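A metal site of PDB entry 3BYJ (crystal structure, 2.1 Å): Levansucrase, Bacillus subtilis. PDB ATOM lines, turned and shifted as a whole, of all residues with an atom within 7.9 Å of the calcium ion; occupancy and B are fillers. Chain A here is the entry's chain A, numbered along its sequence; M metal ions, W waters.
The side-chain amide nitrogen of Gln 272 sits close to the side-chain amide nitrogen of Gln 226 (3.4 Å).
The side-chain amide nitrogen (NE2) of Gln 272 sits at hydrogen-bond distance from the side-chain carboxylate (OE2) of Glu 234, 3.0 Å away.
OD2 of Asp 241 is in hydrogen-bond range of NE2 of Gln 226, 3.0 Å away.
ND2 of Asn 264 sits close to OD1 of Asn 310, at 3.5 Å.
The side-chain amide nitrogen of Asn 310 is in hydrogen-bond range of the side-chain hydroxyl of Thr 265.
ND2 of Asn 264 is in hydrogen-bond range of O of Asp 339 (2.9 Å).
N of Asn 242 sits close to OD2 of Asp 339 (3.1 Å).
The calcium ion is bound by the backbone carbonyl oxygen (O) of Leu 308, the side-chain amide oxygen (OE1) of Gln 272, the side-chain carboxylate (OD1) of Asp 241, water W1, the side-chain amide oxygen (OD1) of Asn 310, the side-chain carboxylate (OD1) of Asp 339 and the side-chain carboxylate (OD2) of Asp 339.
The calcium ion has seven donor atoms within binding distance.
The nearest printed residue that does not touch the calcium ion is Asn 264 (4.1 Å).
Water W1 lies within hydrogen-bond range of the side-chain amide oxygen of Gln 226 (2.7 Å), the backbone carbonyl oxygen of Asn 242 (2.8 Å) and the side-chain amide nitrogen of Asn 264 (3.2 Å).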
ATOM      1  N   GLN A 226      34.983 -32.142  29.759  1.00  0.00           N
ATOM      2  CA  GLN A 226      35.455 -31.376  28.612  1.00  0.00           C
ATOM      3  C   GLN A 226      36.482 -30.345  29.048  1.00  0.00           C
ATOM      4  O   GLN A 226      36.325 -29.701  30.078  1.00  0.00           O
ATOM      5  CB  GLN A 226      34.257 -30.668  27.943  1.00  0.00           C
ATOM      6  CG  GLN A 226      34.533 -30.160  26.524  1.00  0.00           C
ATOM      7  CD  GLN A 226      33.422 -29.286  25.965  1.00  0.00           C
ATOM      8  OE1 GLN A 226      32.898 -28.412  26.649  1.00  0.00           O
ATOM      9  NE2 GLN A 226      33.077 -29.519  24.721  1.00  0.00           N
ATOM     10  N   PHE A 231      36.546 -27.506  23.197  1.00  0.00           N
ATOM     11  CA  PHE A 231      35.676 -26.396  22.821  1.00  0.00           C
ATOM     12  C   PHE A 231      36.246 -25.727  21.563  1.00  0.00           C
ATOM     13  O   PHE A 231      35.508 -25.444  20.590  1.00  0.00           O
ATOM     14  CB  PHE A 231      35.598 -25.412  23.995  1.00  0.00           C
ATOM     15  CG  PHE A 231      34.740 -24.215  23.742  1.00  0.00           C
ATOM     16  CD1 PHE A 231      33.419 -24.351  23.351  1.00  0.00           C
ATOM     17  CD2 PHE A 231      35.255 -22.928  23.941  1.00  0.00           C
ATOM     18  CE1 PHE A 231      32.636 -23.224  23.127  1.00  0.00           C
ATOM     19  CE2 PHE A 231      34.470 -21.818  23.739  1.00  0.00           C
ATOM     20  CZ  PHE A 231      33.153 -21.960  23.327  1.00  0.00           C
ATOM     21  N   GLU A 234      35.646 -27.554  18.236  1.00  0.00           N
ATOM     22  CA  GLU A 234      34.317 -27.348  17.634  1.00  0.00           C
ATOM     23  C   GLU A 234      34.179 -26.041  16.831  1.00  0.00           C
ATOM     24  O   GLU A 234      33.256 -25.909  16.019  1.00  0.00           O
ATOM     25  CB  GLU A 234      33.227 -27.338  18.726  1.00  0.00           C
ATOM     26  CG  GLU A 234      33.153 -28.578  19.615  1.00  0.00           C
ATOM     27  CD  GLU A 234      32.581 -29.805  18.923  1.00  0.00           C
ATOM     28  OE1 GLU A 234      31.992 -29.658  17.826  1.00  0.00           O
ATOM     29  OE2 GLU A 234      32.726 -30.923  19.495  1.00  0.00           O
ATOM     30  N   GLY A 240      28.152 -22.801  18.602  1.00  0.00           N
ATOM     31  CA  GLY A 240      26.981 -23.017  19.447  1.00  0.00           C
ATOM     32  C   GLY A 240      27.263 -23.819  20.717  1.00  0.00           C
ATOM     33  O   GLY A 240      26.405 -23.925  21.595  1.00  0.00           O
ATOM     34  N   ASP A 241      28.466 -24.386  20.833  1.00  0.00           N
ATOM     35  CA  ASP A 241      28.840 -25.158  22.031  1.00  0.00           C
ATOM     36  C   ASP A 241      29.041 -24.186  23.173  1.00  0.00           C
ATOM     37  O   ASP A 241      29.313 -23.019  22.966  1.00  0.00           O
ATOM     38  CB  ASP A 241      30.119 -25.988  21.778  1.00  0.00           C
ATOM     39  CG  ASP A 241      30.301 -27.100  22.793  1.00  0.00           C
ATOM     40  OD1 ASP A 241      29.310 -27.511  23.442  1.00  0.00           O
ATOM     41  OD2 ASP A 241      31.408 -27.662  22.990  1.00  0.00           O
ATOM     42  N   ASN A 242      28.888 -24.686  24.385  1.00  0.00           N
ATOM     43  CA  ASN A 242      28.997 -23.852  25.568  1.00  0.00           C
ATOM     44  C   ASN A 242      29.833 -24.583  26.600  1.00  0.00           C
ATOM     45  O   ASN A 242      29.324 -25.436  27.307  1.00  0.00           O
ATOM     46  CB  ASN A 242      27.595 -23.553  26.110  1.00  0.00           C
ATOM     47  CG  ASN A 242      27.633 -22.742  27.391  1.00  0.00           C
ATOM     48  OD1 ASN A 242      28.695 -22.269  27.802  1.00  0.00           O
ATOM     49  ND2 ASN A 242      26.472 -22.546  27.999  1.00  0.00           N
ATOM     50  N   HIS A 243      31.110 -24.224  26.666  1.00  0.00           N
ATOM     51  CA  HIS A 243      32.046 -24.894  27.533  1.00  0.00           C
ATOM     52  C   HIS A 243      32.018 -24.306  28.936  1.00  0.00           C
ATOM     53  O   HIS A 243      32.076 -23.088  29.125  1.00  0.00           O
ATOM     54  CB  HIS A 243      33.457 -24.808  26.969  1.00  0.00           C
ATOM     55  CG  HIS A 243      34.510 -25.280  27.928  1.00  0.00           C
ATOM     56  ND1 HIS A 243      34.757 -26.618  28.146  1.00  0.00           N
ATOM     57  CD2 HIS A 243      35.356 -24.595  28.726  1.00  0.00           C
ATOM     58  CE1 HIS A 243      35.724 -26.732  29.045  1.00  0.00           C
ATOM     59  NE2 HIS A 243      36.116 -25.529  29.406  1.00  0.00           N
ATOM     60  N   THR A 244      31.955 -25.202  29.913  1.00  0.00           N
ATOM     61  CA  THR A 244      31.901 -24.796  31.306  1.00  0.00           C
ATOM     62  C   THR A 244      32.817 -25.672  32.157  1.00  0.00           C
ATOM     63  O   THR A 244      33.002 -26.869  31.886  1.00  0.00           O
ATOM     64  CB  THR A 244      30.453 -24.831  31.868  1.00  0.00           C
ATOM     65  OG1 THR A 244      30.085 -26.171  32.186  1.00  0.00           O
ATOM     66  CG2 THR A 244      29.418 -24.369  30.826  1.00  0.00           C
ATOM     67  N   ALA A 263      30.329 -28.655  34.984  1.00  0.00           N
ATOM     68  CA  ALA A 263      31.215 -29.072  33.896  1.00  0.00           C
ATOM     69  C   ALA A 263      30.404 -29.478  32.690  1.00  0.00           C
ATOM     70  O   ALA A 263      29.213 -29.200  32.605  1.00  0.00           O
ATOM     71  CB  ALA A 263      32.110 -30.218  34.362  1.00  0.00           C
ATOM     72  N   ASN A 264      31.074 -30.079  31.719  1.00  0.00           N
ATOM     73  CA  ASN A 264      30.443 -30.805  30.644  1.00  0.00           C
ATOM     74  C   ASN A 264      31.148 -32.141  30.504  1.00  0.00           C
ATOM     75  O   ASN A 264      32.315 -32.262  30.889  1.00  0.00           O
ATOM     76  CB  ASN A 264      30.535 -30.014  29.344  1.00  0.00           C
ATOM     77  CG  ASN A 264      29.876 -28.650  29.466  1.00  0.00           C
ATOM     78  OD1 ASN A 264      30.507 -27.679  29.896  1.00  0.00           O
ATOM     79  ND2 ASN A 264      28.601 -28.571  29.083  1.00  0.00           N
ATOM     80  N   THR A 265      30.471 -33.141  29.961  1.00  0.00           N
ATOM     81  CA  THR A 265      31.037 -34.471  29.837  1.00  0.00           C
ATOM     82  C   THR A 265      32.158 -34.518  28.826  1.00  0.00           C
ATOM     83  O   THR A 265      32.301 -33.610  27.996  1.00  0.00           O
ATOM     84  CB  THR A 265      29.992 -35.506  29.413  1.00  0.00           C
ATOM     85  OG1 THR A 265      29.446 -35.141  28.145  1.00  0.00           O
ATOM     86  CG2 THR A 265      28.818 -35.559  30.381  1.00  0.00           C
ATOM     87  N   TYR A 271      29.587 -38.171  25.532  1.00  0.00           N
ATOM     88  CA  TYR A 271      29.934 -36.883  24.975  1.00  0.00           C
ATOM     89  C   TYR A 271      28.816 -36.290  24.112  1.00  0.00           C
ATOM     90  O   TYR A 271      27.914 -37.002  23.636  1.00  0.00           O
ATOM     91  CB  TYR A 271      31.214 -37.024  24.132  1.00  0.00           C
ATOM     92  CG  TYR A 271      31.963 -35.717  23.909  1.00  0.00           C
ATOM     93  CD1 TYR A 271      32.188 -34.837  24.963  1.00  0.00           C
ATOM     94  CD2 TYR A 271      32.456 -35.386  22.639  1.00  0.00           C
ATOM     95  CE1 TYR A 271      32.884 -33.652  24.769  1.00  0.00           C
ATOM     96  CE2 TYR A 271      33.157 -34.202  22.437  1.00  0.00           C
ATOM     97  CZ  TYR A 271      33.362 -33.334  23.515  1.00  0.00           C
ATOM     98  OH  TYR A 271      34.036 -32.148  23.355  1.00  0.00           O
ATOM     99  N   GLN A 272      28.907 -34.975  23.913  1.00  0.00           N
ATOM    100  CA  GLN A 272      28.124 -34.299  22.883  1.00  0.00           C
ATOM    101  C   GLN A 272      28.396 -34.943  21.509  1.00  0.00           C
ATOM    102  O   GLN A 272      29.426 -35.586  21.302  1.00  0.00           O
ATOM    103  CB  GLN A 272      28.453 -32.813  22.855  1.00  0.00           C
ATOM    104  CG  GLN A 272      29.889 -32.480  22.476  1.00  0.00           C
ATOM    105  CD  GLN A 272      30.296 -31.073  22.862  1.00  0.00           C
ATOM    106  OE1 GLN A 272      29.829 -30.556  23.873  1.00  0.00           O
ATOM    107  NE2 GLN A 272      31.155 -30.444  22.058  1.00  0.00           N
ATOM    108  N   GLY A 273      27.460 -34.739  20.590  1.00  0.00           N
ATOM    109  CA  GLY A 273      27.553 -35.252  19.239  1.00  0.00           C
ATOM    110  C   GLY A 273      26.214 -35.727  18.719  1.00  0.00           C
ATOM    111  O   GLY A 273      25.231 -35.837  19.468  1.00  0.00           O
ATOM    112  N   THR A 305      21.291 -27.842  19.090  1.00  0.00           N
ATOM    113  CA  THR A 305      21.432 -27.465  20.492  1.00  0.00           C
ATOM    114  C   THR A 305      21.505 -28.709  21.393  1.00  0.00           C
ATOM    115  O   THR A 305      22.381 -28.822  22.257  1.00  0.00           O
ATOM    116  CB  THR A 305      20.249 -26.548  20.912  1.00  0.00           C
ATOM    117  OG1 THR A 305      20.243 -25.352  20.140  1.00  0.00           O
ATOM    118  CG2 THR A 305      20.400 -26.045  22.352  1.00  0.00           C
ATOM    119  N   ALA A 306      20.588 -29.653  21.169  1.00  0.00           N
ATOM    120  CA  ALA A 306      20.515 -30.890  21.939  1.00  0.00           C
ATOM    121  C   ALA A 306      21.772 -31.762  21.793  1.00  0.00           C
ATOM    122  O   ALA A 306      22.237 -32.363  22.755  1.00  0.00           O
ATOM    123  CB  ALA A 306      19.290 -31.691  21.530  1.00  0.00           C
ATOM    124  N   GLU A 307      22.304 -31.816  20.577  1.00  0.00           N
ATOM    125  CA  GLU A 307      23.503 -32.596  20.282  1.00  0.00           C
ATOM    126  C   GLU A 307      24.691 -32.027  21.069  1.00  0.00           C
ATOM    127  O   GLU A 307      25.514 -32.772  21.603  1.00  0.00           O
ATOM    128  CB  GLU A 307      23.761 -32.577  18.775  1.00  0.00           C
ATOM    129  CG  GLU A 307      22.777 -33.433  17.954  1.00  0.00           C
ATOM    130  CD  GLU A 307      22.830 -33.182  16.460  1.00  0.00           C
ATOM    131  OE1 GLU A 307      23.369 -32.132  16.051  1.00  0.00           O
ATOM    132  OE2 GLU A 307      22.349 -34.042  15.680  1.00  0.00           O
ATOM    133  N   LEU A 308      24.733 -30.695  21.172  1.00  0.00           N
ATOM    134  CA  LEU A 308      25.814 -29.992  21.861  1.00  0.00           C
ATOM    135  C   LEU A 308      25.673 -29.994  23.382  1.00  0.00           C
ATOM    136  O   LEU A 308      26.641 -29.757  24.112  1.00  0.00           O
ATOM    137  CB  LEU A 308      25.845 -28.544  21.401  1.00  0.00           C
ATOM    138  CG  LEU A 308      26.242 -28.319  19.941  1.00  0.00           C
ATOM    139  CD1 LEU A 308      25.771 -26.951  19.468  1.00  0.00           C
ATOM    140  CD2 LEU A 308      27.741 -28.487  19.780  1.00  0.00           C
ATOM    141  N   ALA A 309      24.456 -30.238  23.864  1.00  0.00           N
ATOM    142  CA  ALA A 309      24.142 -30.200  25.283  1.00  0.00           C
ATOM    143  C   ALA A 309      24.689 -31.427  26.003  1.00  0.00           C
ATOM    144  O   ALA A 309      24.227 -32.541  25.784  1.00  0.00           O
ATOM    145  CB  ALA A 309      22.655 -30.097  25.478  1.00  0.00           C
ATOM    146  N   ASN A 310      25.670 -31.214  26.874  1.00  0.00           N
ATOM    147  CA  ASN A 310      26.263 -32.289  27.653  1.00  0.00           C
ATOM    148  C   ASN A 310      26.751 -31.762  28.990  1.00  0.00           C
ATOM    149  O   ASN A 310      27.864 -32.035  29.417  1.00  0.00           O
ATOM    150  CB  ASN A 310      27.360 -32.999  26.859  1.00  0.00           C
ATOM    151  CG  ASN A 310      28.591 -32.161  26.659  1.00  0.00           C
ATOM    152  OD1 ASN A 310      28.513 -30.932  26.520  1.00  0.00           O
ATOM    153  ND2 ASN A 310      29.748 -32.808  26.653  1.00  0.00           N
ATOM    154  N   GLY A 311      25.881 -31.008  29.657  1.00  0.00           N
ATOM    155  CA  GLY A 311      26.139 -30.482  30.986  1.00  0.00           C
ATOM    156  C   GLY A 311      26.362 -31.613  31.957  1.00  0.00           C
ATOM    157  O   GLY A 311      25.871 -32.731  31.767  1.00  0.00           O
ATOM    158  N   THR A 338      20.385 -29.655  28.316  1.00  0.00           N
ATOM    159  CA  THR A 338      21.137 -28.415  28.324  1.00  0.00           C
ATOM    160  C   THR A 338      22.618 -28.630  28.536  1.00  0.00           C
ATOM    161  O   THR A 338      23.040 -29.633  29.105  1.00  0.00           O
ATOM    162  CB  THR A 338      20.574 -27.470  29.410  1.00  0.00           C
ATOM    163  OG1 THR A 338      21.311 -26.243  29.433  1.00  0.00           O
ATOM    164  CG2 THR A 338      20.752 -28.058  30.795  1.00  0.00           C
ATOM    165  N   ASP A 339      23.395 -27.646  28.069  1.00  0.00           N
ATOM    166  CA  ASP A 339      24.843 -27.569  28.259  1.00  0.00           C
ATOM    167  C   ASP A 339      25.241 -26.843  29.552  1.00  0.00           C
ATOM    168  O   ASP A 339      26.434 -26.769  29.886  1.00  0.00           O
ATOM    169  CB  ASP A 339      25.457 -26.767  27.108  1.00  0.00           C
ATOM    170  CG  ASP A 339      26.575 -27.482  26.399  1.00  0.00           C
ATOM    171  OD1 ASP A 339      27.034 -28.541  26.863  1.00  0.00           O
ATOM    172  OD2 ASP A 339      27.079 -27.030  25.346  1.00  0.00           O
ATOM    173  N   GLU A 340      24.266 -26.260  30.253  1.00  0.00           N
ATOM    174  CA  GLU A 340      24.572 -25.302  31.309  1.00  0.00           C
ATOM    175  C   GLU A 340      23.783 -25.556  32.585  1.00  0.00           C
ATOM    176  O   GLU A 340      22.632 -25.105  32.723  1.00  0.00           O
ATOM    177  CB  GLU A 340      24.324 -23.878  30.812  1.00  0.00           C
ATOM    178  CG  GLU A 340      24.956 -22.800  31.693  1.00  0.00           C
ATOM    179  CD  GLU A 340      24.802 -21.417  31.115  1.00  0.00           C
ATOM    180  OE1 GLU A 340      25.716 -20.990  30.392  1.00  0.00           O
ATOM    181  OE2 GLU A 340      23.751 -20.766  31.369  1.00  0.00           O
HETATM  182 CA    CA M   1      28.597 -29.008  25.012  1.00  0.00          CA
HETATM  183  O   HOH W   1      30.272 -27.967  26.444  1.00  0.00           O
